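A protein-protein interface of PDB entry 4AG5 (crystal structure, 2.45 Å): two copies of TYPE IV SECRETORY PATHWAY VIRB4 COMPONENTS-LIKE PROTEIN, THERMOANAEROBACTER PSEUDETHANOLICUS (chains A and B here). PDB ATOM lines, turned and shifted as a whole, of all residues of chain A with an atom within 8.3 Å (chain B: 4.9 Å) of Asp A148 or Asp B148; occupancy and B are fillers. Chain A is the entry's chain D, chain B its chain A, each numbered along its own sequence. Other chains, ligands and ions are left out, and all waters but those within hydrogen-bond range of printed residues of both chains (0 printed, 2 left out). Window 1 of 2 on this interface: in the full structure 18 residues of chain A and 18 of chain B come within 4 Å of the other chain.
OE1 of Glu B152 sits close to OE2 of Glu A152, at 3.1 Å.
O of Ala A145 sits at hydrogen-bond distance from OH of Tyr A194, 2.7 Å away. The backbone carbonyl oxygen of Ala B145 lies within hydrogen-bond range of the side-chain hydroxyl of Tyr B194 (2.6 Å).
Trp B161 touches Ala A144 (CH2 to O, 3.8 Å). Ala A145 touches Trp B161. OD1 of Asp B148 touches OD1 of Asp A148, 3.7 Å away. Asp A148 touches Val B151. CZ2 of Trp B161 touches CB of Asp A148, at 3.6 Å. Val A151 touches Asp B148 (CG1 to OD1, 3.2 Å). Ala B144 touches Trp A161. OD2 of Asp B148 touches NE1 of Trp A161, at 3.8 Å. Trp A161 touches Tyr B194. CE2 of Tyr A194 touches CD1 of Trp B161, 3.97 Å away.
Asp A148 touches just these residues of chain B: Asp B148 (3.7 Å), Val B151 (3.5 Å) and Trp B161 (3.6 Å). Asp B148 touches three residues of chain A. Printed residues of chain A within 4 Å of Val B151: Asp A148. Of the printed residues of chain B, Trp A161 touches Ala B144 (3.9 Å), Asp B148 (3.8 Å) and Tyr B194 (3.6 Å). Printed residues of chain B within 4 Å of Val A151: Asp B148 (3.2 Å). Printed residues of chain B within 4 Å of Ala A144: Trp B161. Of the printed residues of chain B, Glu A152 touches Glu B152 (3.1 Å). Leu A120 touches none of the printed residues of chain B.
Of the 24 printed residues of chain A, 7 touch a printed residue of chain B. Printed residues of chain A that touch a printed residue of chain B: Ala A144, Ala A145, Asp A148, Val A151, Glu A152, Trp A161 and Tyr A194. Hydrophobic or aromatic side chains of chain A within 4 Å of the printed part of chain B: Ala A144, Val A151, Trp A161 and Tyr A194. Of the 12 printed residues of chain B, 6 touch a printed residue of chain A. Printed residues of chain B that touch a printed residue of chain A: Ala B144, Asp B148, Val B151, Glu B152, Trp B161 and Tyr B194. Hydrophobic or aromatic side chains of chain B that line the printed part of chain A: Val B151, Trp B161 and Tyr B194.
Ala A144 touches Trp B161, and with the chains exchanged Trp A161 touches Ala B144. Ala A145 touches Trp B161, but with the chains exchanged Trp A161 does not touch Ala B145 (4.2 Å). Asp A148 touches Trp B161, and with the chains exchanged Trp A161 touches Asp B148. Trp A161 touches Tyr B194, and with the chains exchanged Tyr A194 touches Trp B161. Positions printed for both chains: 144, 145, 146, 147, 148, 149, 150, 151, 152, 161, 182 and 194.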
ATOM      1  N   LEU A 120      -8.041 -13.597  16.782  1.00  0.00           N
ATOM      2  CA  LEU A 120      -7.870 -12.431  17.628  1.00  0.00           C
ATOM      3  C   LEU A 120      -9.125 -12.196  18.453  1.00  0.00           C
ATOM      4  O   LEU A 120      -9.034 -11.905  19.644  1.00  0.00           O
ATOM      5  CB  LEU A 120      -7.512 -11.186  16.802  1.00  0.00           C
ATOM      6  CG  LEU A 120      -7.276  -9.889  17.594  1.00  0.00           C
ATOM      7  CD1 LEU A 120      -6.203 -10.085  18.665  1.00  0.00           C
ATOM      8  CD2 LEU A 120      -6.910  -8.714  16.689  1.00  0.00           C
ATOM      9  N   ILE A 124      -9.351 -12.482  22.491  1.00  0.00           N
ATOM     10  CA  ILE A 124      -9.731 -11.219  23.152  1.00  0.00           C
ATOM     11  C   ILE A 124     -10.634 -11.482  24.368  1.00  0.00           C
ATOM     12  O   ILE A 124     -10.572 -10.775  25.388  1.00  0.00           O
ATOM     13  CB  ILE A 124     -10.464 -10.222  22.184  1.00  0.00           C
ATOM     14  CG1 ILE A 124      -9.470  -9.513  21.256  1.00  0.00           C
ATOM     15  CG2 ILE A 124     -11.274  -9.200  22.969  1.00  0.00           C
ATOM     16  CD1 ILE A 124      -8.326  -8.858  21.973  1.00  0.00           C
ATOM     17  N   THR A 141     -17.255  -0.345  31.843  1.00  0.00           N
ATOM     18  CA  THR A 141     -16.603   0.663  31.019  1.00  0.00           C
ATOM     19  C   THR A 141     -15.103   0.388  30.949  1.00  0.00           C
ATOM     20  O   THR A 141     -14.501   0.461  29.886  1.00  0.00           O
ATOM     21  CB  THR A 141     -16.833   2.089  31.574  1.00  0.00           C
ATOM     22  OG1 THR A 141     -18.023   2.644  31.007  1.00  0.00           O
ATOM     23  CG2 THR A 141     -15.657   3.011  31.231  1.00  0.00           C
ATOM     24  N   GLU A 142     -14.496   0.062  32.086  1.00  0.00           N
ATOM     25  CA  GLU A 142     -13.063  -0.203  32.099  1.00  0.00           C
ATOM     26  C   GLU A 142     -12.733  -1.490  31.348  1.00  0.00           C
ATOM     27  O   GLU A 142     -11.710  -1.580  30.675  1.00  0.00           O
ATOM     28  CB  GLU A 142     -12.534  -0.242  33.530  1.00  0.00           C
ATOM     29  CG  GLU A 142     -12.545   1.115  34.210  1.00  0.00           C
ATOM     30  CD  GLU A 142     -12.208   1.016  35.687  1.00  0.00           C
ATOM     31  OE1 GLU A 142     -12.393  -0.082  36.260  1.00  0.00           O
ATOM     32  OE2 GLU A 142     -11.763   2.031  36.269  1.00  0.00           O
ATOM     33  N   LYS A 143     -13.616  -2.475  31.455  1.00  0.00           N
ATOM     34  CA  LYS A 143     -13.476  -3.719  30.709  1.00  0.00           C
ATOM     35  C   LYS A 143     -13.485  -3.460  29.203  1.00  0.00           C
ATOM     36  O   LYS A 143     -12.615  -3.950  28.469  1.00  0.00           O
ATOM     37  CB  LYS A 143     -14.596  -4.690  31.081  1.00  0.00           C
ATOM     38  CG  LYS A 143     -14.681  -4.984  32.563  1.00  0.00           C
ATOM     39  CD  LYS A 143     -15.735  -6.029  32.866  1.00  0.00           C
ATOM     40  CE  LYS A 143     -15.488  -6.676  34.223  1.00  0.00           C
ATOM     41  NZ  LYS A 143     -16.284  -7.920  34.364  1.00  0.00           N
ATOM     42  N   ALA A 144     -14.461  -2.680  28.746  1.00  0.00           N
ATOM     43  CA  ALA A 144     -14.564  -2.337  27.329  1.00  0.00           C
ATOM     44  C   ALA A 144     -13.345  -1.545  26.875  1.00  0.00           C
ATOM     45  O   ALA A 144     -12.761  -1.821  25.818  1.00  0.00           O
ATOM     46  CB  ALA A 144     -15.856  -1.561  27.057  1.00  0.00           C
ATOM     47  N   ALA A 145     -12.956  -0.564  27.686  1.00  0.00           N
ATOM     48  CA  ALA A 145     -11.769   0.245  27.417  1.00  0.00           C
ATOM     49  C   ALA A 145     -10.561  -0.654  27.199  1.00  0.00           C
ATOM     50  O   ALA A 145      -9.845  -0.510  26.207  1.00  0.00           O
ATOM     51  CB  ALA A 145     -11.516   1.224  28.549  1.00  0.00           C
ATOM     52  N   LEU A 146     -10.357  -1.597  28.121  1.00  0.00           N
ATOM     53  CA  LEU A 146      -9.278  -2.578  28.003  1.00  0.00           C
ATOM     54  C   LEU A 146      -9.359  -3.382  26.708  1.00  0.00           C
ATOM     55  O   LEU A 146      -8.387  -3.478  25.976  1.00  0.00           O
ATOM     56  CB  LEU A 146      -9.280  -3.548  29.190  1.00  0.00           C
ATOM     57  CG  LEU A 146      -8.117  -4.563  29.167  1.00  0.00           C
ATOM     58  CD1 LEU A 146      -6.859  -3.954  29.794  1.00  0.00           C
ATOM     59  CD2 LEU A 146      -8.488  -5.867  29.844  1.00  0.00           C
ATOM     60  N   GLU A 147     -10.510  -3.981  26.438  1.00  0.00           N
ATOM     61  CA  GLU A 147     -10.667  -4.781  25.230  1.00  0.00           C
ATOM     62  C   GLU A 147     -10.260  -3.995  23.974  1.00  0.00           C
ATOM     63  O   GLU A 147      -9.495  -4.475  23.111  1.00  0.00           O
ATOM     64  CB  GLU A 147     -12.114  -5.258  25.120  1.00  0.00           C
ATOM     65  N   ASP A 148     -10.762  -2.771  23.877  1.00  0.00           N
ATOM     66  CA  ASP A 148     -10.428  -1.941  22.721  1.00  0.00           C
ATOM     67  C   ASP A 148      -8.921  -1.681  22.680  1.00  0.00           C
ATOM     68  O   ASP A 148      -8.281  -1.762  21.617  1.00  0.00           O
ATOM     69  CB  ASP A 148     -11.213  -0.625  22.728  1.00  0.00           C
ATOM     70  CG  ASP A 148     -10.924   0.223  21.502  1.00  0.00           C
ATOM     71  OD1 ASP A 148     -11.444  -0.115  20.419  1.00  0.00           O
ATOM     72  OD2 ASP A 148     -10.170   1.215  21.611  1.00  0.00           O
ATOM     73  N   ALA A 149      -8.349  -1.382  23.841  1.00  0.00           N
ATOM     74  CA  ALA A 149      -6.907  -1.208  23.923  1.00  0.00           C
ATOM     75  C   ALA A 149      -6.185  -2.433  23.358  1.00  0.00           C
ATOM     76  O   ALA A 149      -5.217  -2.302  22.621  1.00  0.00           O
ATOM     77  CB  ALA A 149      -6.478  -0.932  25.356  1.00  0.00           C
ATOM     78  N   LEU A 150      -6.666  -3.623  23.690  1.00  0.00           N
ATOM     79  CA  LEU A 150      -6.076  -4.834  23.149  1.00  0.00           C
ATOM     80  C   LEU A 150      -6.068  -4.760  21.635  1.00  0.00           C
ATOM     81  O   LEU A 150      -5.016  -4.874  20.993  1.00  0.00           O
ATOM     82  CB  LEU A 150      -6.824  -6.075  23.642  1.00  0.00           C
ATOM     83  CG  LEU A 150      -6.618  -6.398  25.125  1.00  0.00           C
ATOM     84  CD1 LEU A 150      -7.443  -7.600  25.548  1.00  0.00           C
ATOM     85  CD2 LEU A 150      -5.139  -6.605  25.430  1.00  0.00           C
ATOM     86  N   VAL A 151      -7.242  -4.540  21.055  1.00  0.00           N
ATOM     87  CA  VAL A 151      -7.313  -4.475  19.595  1.00  0.00           C
ATOM     88  C   VAL A 151      -6.293  -3.493  18.994  1.00  0.00           C
ATOM     89  O   VAL A 151      -5.602  -3.831  18.028  1.00  0.00           O
ATOM     90  CB  VAL A 151      -8.751  -4.184  19.091  1.00  0.00           C
ATOM     91  CG1 VAL A 151      -8.738  -3.763  17.627  1.00  0.00           C
ATOM     92  CG2 VAL A 151      -9.641  -5.412  19.290  1.00  0.00           C
ATOM     93  N   GLU A 152      -6.185  -2.296  19.579  1.00  0.00           N
ATOM     94  CA  GLU A 152      -5.280  -1.256  19.058  1.00  0.00           C
ATOM     95  C   GLU A 152      -3.792  -1.586  19.207  1.00  0.00           C
ATOM     96  O   GLU A 152      -2.982  -1.358  18.294  1.00  0.00           O
ATOM     97  CB  GLU A 152      -5.562   0.105  19.712  1.00  0.00           C
ATOM     98  CG  GLU A 152      -6.814   0.795  19.216  1.00  0.00           C
ATOM     99  CD  GLU A 152      -6.924   0.792  17.703  1.00  0.00           C
ATOM    100  OE1 GLU A 152      -5.965   1.233  17.044  1.00  0.00           O
ATOM    101  OE2 GLU A 152      -7.962   0.335  17.179  1.00  0.00           O
ATOM    102  N   VAL A 153      -3.434  -2.094  20.381  1.00  0.00           N
ATOM    103  CA  VAL A 153      -2.074  -2.539  20.645  1.00  0.00           C
ATOM    104  C   VAL A 153      -1.698  -3.619  19.633  1.00  0.00           C
ATOM    105  O   VAL A 153      -0.560  -3.684  19.174  1.00  0.00           O
ATOM    106  CB  VAL A 153      -1.925  -3.042  22.105  1.00  0.00           C
ATOM    107  CG1 VAL A 153      -1.325  -4.437  22.155  1.00  0.00           C
ATOM    108  CG2 VAL A 153      -1.103  -2.059  22.922  1.00  0.00           C
ATOM    109  N   TYR A 154      -2.668  -4.449  19.266  1.00  0.00           N
ATOM    110  CA  TYR A 154      -2.439  -5.453  18.230  1.00  0.00           C
ATOM    111  C   TYR A 154      -2.239  -4.839  16.845  1.00  0.00           C
ATOM    112  O   TYR A 154      -1.292  -5.199  16.138  1.00  0.00           O
ATOM    113  CB  TYR A 154      -3.588  -6.438  18.188  1.00  0.00           C
ATOM    114  CG  TYR A 154      -3.542  -7.508  19.247  1.00  0.00           C
ATOM    115  CD1 TYR A 154      -2.570  -8.500  19.225  1.00  0.00           C
ATOM    116  CD2 TYR A 154      -4.501  -7.550  20.253  1.00  0.00           C
ATOM    117  CE1 TYR A 154      -2.551  -9.498  20.178  1.00  0.00           C
ATOM    118  CE2 TYR A 154      -4.487  -8.544  21.218  1.00  0.00           C
ATOM    119  CZ  TYR A 154      -3.513  -9.514  21.176  1.00  0.00           C
ATOM    120  OH  TYR A 154      -3.510 -10.498  22.140  1.00  0.00           O
ATOM    121  N   LYS A 155      -3.133  -3.921  16.458  1.00  0.00           N
ATOM    122  CA  LYS A 155      -3.014  -3.239  15.167  1.00  0.00           C
ATOM    123  C   LYS A 155      -1.642  -2.569  15.009  1.00  0.00           C
ATOM    124  O   LYS A 155      -1.030  -2.631  13.938  1.00  0.00           O
ATOM    125  CB  LYS A 155      -4.136  -2.213  14.966  1.00  0.00           C
ATOM    126  N   TRP A 161      -7.593  -8.704  12.132  1.00  0.00           N
ATOM    127  CA  TRP A 161      -8.657  -9.682  12.297  1.00  0.00           C
ATOM    128  C   TRP A 161      -8.436 -10.886  11.408  1.00  0.00           C
ATOM    129  O   TRP A 161      -8.838 -11.995  11.756  1.00  0.00           O
ATOM    130  CB  TRP A 161     -10.025  -9.065  11.996  1.00  0.00           C
ATOM    131  CG  TRP A 161     -10.377  -7.963  12.926  1.00  0.00           C
ATOM    132  CD1 TRP A 161     -10.219  -6.627  12.709  1.00  0.00           C
ATOM    133  CD2 TRP A 161     -10.925  -8.094  14.240  1.00  0.00           C
ATOM    134  NE1 TRP A 161     -10.634  -5.921  13.808  1.00  0.00           N
ATOM    135  CE2 TRP A 161     -11.078  -6.802  14.759  1.00  0.00           C
ATOM    136  CE3 TRP A 161     -11.291  -9.183  15.029  1.00  0.00           C
ATOM    137  CZ2 TRP A 161     -11.593  -6.566  16.026  1.00  0.00           C
ATOM    138  CZ3 TRP A 161     -11.799  -8.942  16.294  1.00  0.00           C
ATOM    139  CH2 TRP A 161     -11.946  -7.645  16.775  1.00  0.00           C
ATOM    140  N   LEU A 179       0.475  -2.604  26.033  1.00  0.00           N
ATOM    141  CA  LEU A 179      -0.893  -2.349  26.456  1.00  0.00           C
ATOM    142  C   LEU A 179      -0.907  -1.254  27.522  1.00  0.00           C
ATOM    143  O   LEU A 179      -1.797  -0.392  27.541  1.00  0.00           O
ATOM    144  CB  LEU A 179      -1.530  -3.621  26.998  1.00  0.00           C
ATOM    145  CG  LEU A 179      -2.893  -3.505  27.682  1.00  0.00           C
ATOM    146  CD1 LEU A 179      -3.994  -3.170  26.681  1.00  0.00           C
ATOM    147  CD2 LEU A 179      -3.213  -4.791  28.418  1.00  0.00           C
ATOM    148  N   TYR A 182       0.066   2.068  25.761  1.00  0.00           N
ATOM    149  CA  TYR A 182      -1.149   2.480  25.097  1.00  0.00           C
ATOM    150  C   TYR A 182      -2.088   3.158  26.087  1.00  0.00           C
ATOM    151  O   TYR A 182      -2.506   4.291  25.878  1.00  0.00           O
ATOM    152  CB  TYR A 182      -1.874   1.314  24.399  1.00  0.00           C
ATOM    153  CG  TYR A 182      -3.114   1.813  23.691  1.00  0.00           C
ATOM    154  CD1 TYR A 182      -3.021   2.440  22.456  1.00  0.00           C
ATOM    155  CD2 TYR A 182      -4.364   1.727  24.286  1.00  0.00           C
ATOM    156  CE1 TYR A 182      -4.135   2.928  21.819  1.00  0.00           C
ATOM    157  CE2 TYR A 182      -5.488   2.217  23.655  1.00  0.00           C
ATOM    158  CZ  TYR A 182      -5.367   2.818  22.424  1.00  0.00           C
ATOM    159  OH  TYR A 182      -6.481   3.309  21.777  1.00  0.00           O
ATOM    160  N   CYS A 183      -2.429   2.473  27.168  1.00  0.00           N
ATOM    161  CA  CYS A 183      -3.439   3.021  28.067  1.00  0.00           C
ATOM    162  C   CYS A 183      -2.987   4.299  28.742  1.00  0.00           C
ATOM    163  O   CYS A 183      -3.794   5.167  29.039  1.00  0.00           O
ATOM    164  CB  CYS A 183      -3.833   2.005  29.128  1.00  0.00           C
ATOM    165  SG  CYS A 183      -4.572   0.571  28.423  1.00  0.00           S
ATOM    166  N   LYS A 186      -3.721   6.892  26.179  1.00  0.00           N
ATOM    167  CA  LYS A 186      -5.153   7.128  26.105  1.00  0.00           C
ATOM    168  C   LYS A 186      -5.664   7.883  27.333  1.00  0.00           C
ATOM    169  O   LYS A 186      -6.639   8.634  27.244  1.00  0.00           O
ATOM    170  CB  LYS A 186      -5.920   5.810  25.942  1.00  0.00           C
ATOM    171  CG  LYS A 186      -6.373   5.507  24.515  1.00  0.00           C
ATOM    172  CD  LYS A 186      -7.619   6.308  24.133  1.00  0.00           C
ATOM    173  N   TYR A 194      -9.591   5.555  31.470  1.00  0.00           N
ATOM    174  CA  TYR A 194      -8.264   4.920  31.352  1.00  0.00           C
ATOM    175  C   TYR A 194      -7.265   5.122  32.501  1.00  0.00           C
ATOM    176  O   TYR A 194      -6.349   4.321  32.676  1.00  0.00           O
ATOM    177  CB  TYR A 194      -7.595   5.309  30.030  1.00  0.00           C
ATOM    178  CG  TYR A 194      -8.034   4.461  28.868  1.00  0.00           C
ATOM    179  CD1 TYR A 194      -7.843   3.085  28.879  1.00  0.00           C
ATOM    180  CD2 TYR A 194      -8.639   5.029  27.763  1.00  0.00           C
ATOM    181  CE1 TYR A 194      -8.239   2.300  27.822  1.00  0.00           C
ATOM    182  CE2 TYR A 194      -9.047   4.248  26.697  1.00  0.00           C
ATOM    183  CZ  TYR A 194      -8.844   2.886  26.733  1.00  0.00           C
ATOM    184  OH  TYR A 194      -9.249   2.117  25.670  1.00  0.00           O
ATOM    185  N   LEU A 197      -7.054   2.240  34.915  1.00  0.00           N
ATOM    186  CA  LEU A 197      -6.695   1.029  34.187  1.00  0.00           C
ATOM    187  C   LEU A 197      -5.198   1.033  33.920  1.00  0.00           C
ATOM    188  O   LEU A 197      -4.557  -0.018  33.917  1.00  0.00           O
ATOM    189  CB  LEU A 197      -7.481   0.923  32.876  1.00  0.00           C
ATOM    190  CG  LEU A 197      -7.429  -0.410  32.122  1.00  0.00           C
ATOM    191  CD1 LEU A 197      -7.789  -1.566  33.031  1.00  0.00           C
ATOM    192  CD2 LEU A 197      -8.355  -0.376  30.919  1.00  0.00           C
ATOM    193  N   ALA B 144     -17.965  -8.320  16.815  1.00  0.00           N
ATOM    194  CA  ALA B 144     -16.865  -7.649  17.492  1.00  0.00           C
ATOM    195  C   ALA B 144     -16.029  -6.787  16.549  1.00  0.00           C
ATOM    196  O   ALA B 144     -15.390  -5.833  16.984  1.00  0.00           O
ATOM    197  CB  ALA B 144     -15.993  -8.660  18.225  1.00  0.00           C
ATOM    198  N   ALA B 145     -16.016  -7.126  15.266  1.00  0.00           N
ATOM    199  CA  ALA B 145     -15.383  -6.261  14.283  1.00  0.00           C
ATOM    200  C   ALA B 145     -16.240  -4.992  14.103  1.00  0.00           C
ATOM    201  O   ALA B 145     -15.733  -3.911  13.785  1.00  0.00           O
ATOM    202  CB  ALA B 145     -15.248  -6.979  12.969  1.00  0.00           C
ATOM    203  N   LEU B 146     -17.545  -5.152  14.286  1.00  0.00           N
ATOM    204  CA  LEU B 146     -18.477  -4.061  14.145  1.00  0.00           C
ATOM    205  C   LEU B 146     -18.336  -3.139  15.338  1.00  0.00           C
ATOM    206  O   LEU B 146     -18.284  -1.923  15.180  1.00  0.00           O
ATOM    207  CB  LEU B 146     -19.901  -4.582  14.065  1.00  0.00           C
ATOM    208  CG  LEU B 146     -20.962  -3.504  13.876  1.00  0.00           C
ATOM    209  CD1 LEU B 146     -20.839  -2.945  12.485  1.00  0.00           C
ATOM    210  CD2 LEU B 146     -22.335  -4.067  14.094  1.00  0.00           C
ATOM    211  N   GLU B 147     -18.281  -3.716  16.533  1.00  0.00           N
ATOM    212  CA  GLU B 147     -18.013  -2.922  17.728  1.00  0.00           C
ATOM    213  C   GLU B 147     -16.675  -2.211  17.636  1.00  0.00           C
ATOM    214  O   GLU B 147     -16.483  -1.157  18.238  1.00  0.00           O
ATOM    215  CB  GLU B 147     -18.044  -3.782  18.988  1.00  0.00           C
ATOM    216  CG  GLU B 147     -19.431  -4.201  19.403  1.00  0.00           C
ATOM    217  CD  GLU B 147     -19.448  -4.845  20.769  1.00  0.00           C
ATOM    218  OE1 GLU B 147     -18.589  -4.486  21.603  1.00  0.00           O
ATOM    219  OE2 GLU B 147     -20.320  -5.711  21.003  1.00  0.00           O
ATOM    220  N   ASP B 148     -15.744  -2.782  16.885  1.00  0.00           N
ATOM    221  CA  ASP B 148     -14.436  -2.161  16.765  1.00  0.00           C
ATOM    222  C   ASP B 148     -14.490  -1.019  15.759  1.00  0.00           C
ATOM    223  O   ASP B 148     -13.923   0.053  15.981  1.00  0.00           O
ATOM    224  CB  ASP B 148     -13.364  -3.168  16.356  1.00  0.00           C
ATOM    225  CG  ASP B 148     -11.982  -2.531  16.247  1.00  0.00           C
ATOM    226  OD1 ASP B 148     -11.453  -2.138  17.306  1.00  0.00           O
ATOM    227  OD2 ASP B 148     -11.436  -2.414  15.119  1.00  0.00           O
ATOM    228  N   ALA B 149     -15.163  -1.256  14.643  1.00  0.00           N
ATOM    229  CA  ALA B 149     -15.299  -0.226  13.635  1.00  0.00           C
ATOM    230  C   ALA B 149     -16.064   0.973  14.229  1.00  0.00           C
ATOM    231  O   ALA B 149     -15.754   2.133  13.944  1.00  0.00           O
ATOM    232  CB  ALA B 149     -16.003  -0.786  12.419  1.00  0.00           C
ATOM    233  N   LEU B 150     -17.045   0.672  15.075  1.00  0.00           N
ATOM    234  CA  LEU B 150     -17.843   1.675  15.753  1.00  0.00           C
ATOM    235  C   LEU B 150     -16.985   2.636  16.582  1.00  0.00           C
ATOM    236  O   LEU B 150     -17.054   3.855  16.403  1.00  0.00           O
ATOM    237  CB  LEU B 150     -18.908   0.998  16.621  1.00  0.00           C
ATOM    238  CG  LEU B 150     -20.144   0.584  15.815  1.00  0.00           C
ATOM    239  CD1 LEU B 150     -21.134  -0.221  16.638  1.00  0.00           C
ATOM    240  CD2 LEU B 150     -20.818   1.831  15.210  1.00  0.00           C
ATOM    241  N   VAL B 151     -16.169   2.088  17.477  1.00  0.00           N
ATOM    242  CA  VAL B 151     -15.307   2.900  18.333  1.00  0.00           C
ATOM    243  C   VAL B 151     -14.335   3.701  17.498  1.00  0.00           C
ATOM    244  O   VAL B 151     -13.971   4.828  17.855  1.00  0.00           O
ATOM    245  CB  VAL B 151     -14.502   2.016  19.323  1.00  0.00           C
ATOM    246  CG1 VAL B 151     -13.310   2.786  19.918  1.00  0.00           C
ATOM    247  CG2 VAL B 151     -15.408   1.468  20.408  1.00  0.00           C
ATOM    248  N   GLU B 152     -13.901   3.115  16.388  1.00  0.00           N
ATOM    249  CA  GLU B 152     -12.885   3.740  15.535  1.00  0.00           C
ATOM    250  C   GLU B 152     -13.498   4.888  14.747  1.00  0.00           C
ATOM    251  O   GLU B 152     -12.888   5.939  14.566  1.00  0.00           O
ATOM    252  CB  GLU B 152     -12.279   2.704  14.582  1.00  0.00           C
ATOM    253  CG  GLU B 152     -10.812   2.921  14.276  1.00  0.00           C
ATOM    254  CD  GLU B 152     -10.009   3.160  15.526  1.00  0.00           C
ATOM    255  OE1 GLU B 152     -10.138   2.357  16.478  1.00  0.00           O
ATOM    256  OE2 GLU B 152      -9.269   4.166  15.562  1.00  0.00           O
ATOM    257  N   TRP B 161     -13.955   8.071  24.895  1.00  0.00           N
ATOM    258  CA  TRP B 161     -14.571   7.349  26.009  1.00  0.00           C
ATOM    259  C   TRP B 161     -15.083   8.247  27.122  1.00  0.00           C
ATOM    260  O   TRP B 161     -16.021   7.895  27.820  1.00  0.00           O
ATOM    261  CB  TRP B 161     -13.593   6.318  26.580  1.00  0.00           C
ATOM    262  CG  TRP B 161     -13.149   5.331  25.555  1.00  0.00           C
ATOM    263  CD1 TRP B 161     -12.180   5.512  24.614  1.00  0.00           C
ATOM    264  CD2 TRP B 161     -13.668   4.015  25.352  1.00  0.00           C
ATOM    265  NE1 TRP B 161     -12.063   4.389  23.836  1.00  0.00           N
ATOM    266  CE2 TRP B 161     -12.965   3.453  24.272  1.00  0.00           C
ATOM    267  CE3 TRP B 161     -14.665   3.261  25.971  1.00  0.00           C
ATOM    268  CZ2 TRP B 161     -13.224   2.170  23.805  1.00  0.00           C
ATOM    269  CZ3 TRP B 161     -14.920   1.983  25.504  1.00  0.00           C
ATOM    270  CH2 TRP B 161     -14.201   1.451  24.433  1.00  0.00           C
ATOM    271  N   TYR B 182     -15.603   2.937   6.655  1.00  0.00           N
ATOM    272  CA  TYR B 182     -14.487   2.410   7.414  1.00  0.00           C
ATOM    273  C   TYR B 182     -14.422   0.891   7.251  1.00  0.00           C
ATOM    274  O   TYR B 182     -13.346   0.309   7.125  1.00  0.00           O
ATOM    275  CB  TYR B 182     -14.670   2.776   8.882  1.00  0.00           C
ATOM    276  CG  TYR B 182     -13.714   2.094   9.829  1.00  0.00           C
ATOM    277  CD1 TYR B 182     -13.905   0.778  10.211  1.00  0.00           C
ATOM    278  CD2 TYR B 182     -12.636   2.778  10.359  1.00  0.00           C
ATOM    279  CE1 TYR B 182     -13.041   0.159  11.082  1.00  0.00           C
ATOM    280  CE2 TYR B 182     -11.777   2.174  11.233  1.00  0.00           C
ATOM    281  CZ  TYR B 182     -11.979   0.864  11.588  1.00  0.00           C
ATOM    282  OH  TYR B 182     -11.110   0.265  12.459  1.00  0.00           O
ATOM    283  N   TYR B 194     -14.561  -8.603   7.596  1.00  0.00           N
ATOM    284  CA  TYR B 194     -15.337  -7.397   7.303  1.00  0.00           C
ATOM    285  C   TYR B 194     -16.092  -7.462   5.988  1.00  0.00           C
ATOM    286  O   TYR B 194     -17.139  -6.833   5.833  1.00  0.00           O
ATOM    287  CB  TYR B 194     -14.431  -6.161   7.299  1.00  0.00           C
ATOM    288  CG  TYR B 194     -14.196  -5.578   8.663  1.00  0.00           C
ATOM    289  CD1 TYR B 194     -15.205  -4.897   9.324  1.00  0.00           C
ATOM    290  CD2 TYR B 194     -12.960  -5.690   9.287  1.00  0.00           C
ATOM    291  CE1 TYR B 194     -14.993  -4.347  10.591  1.00  0.00           C
ATOM    292  CE2 TYR B 194     -12.739  -5.143  10.543  1.00  0.00           C
ATOM    293  CZ  TYR B 194     -13.761  -4.481  11.186  1.00  0.00           C
ATOM    294  OH  TYR B 194     -13.550  -3.954  12.429  1.00  0.00           O
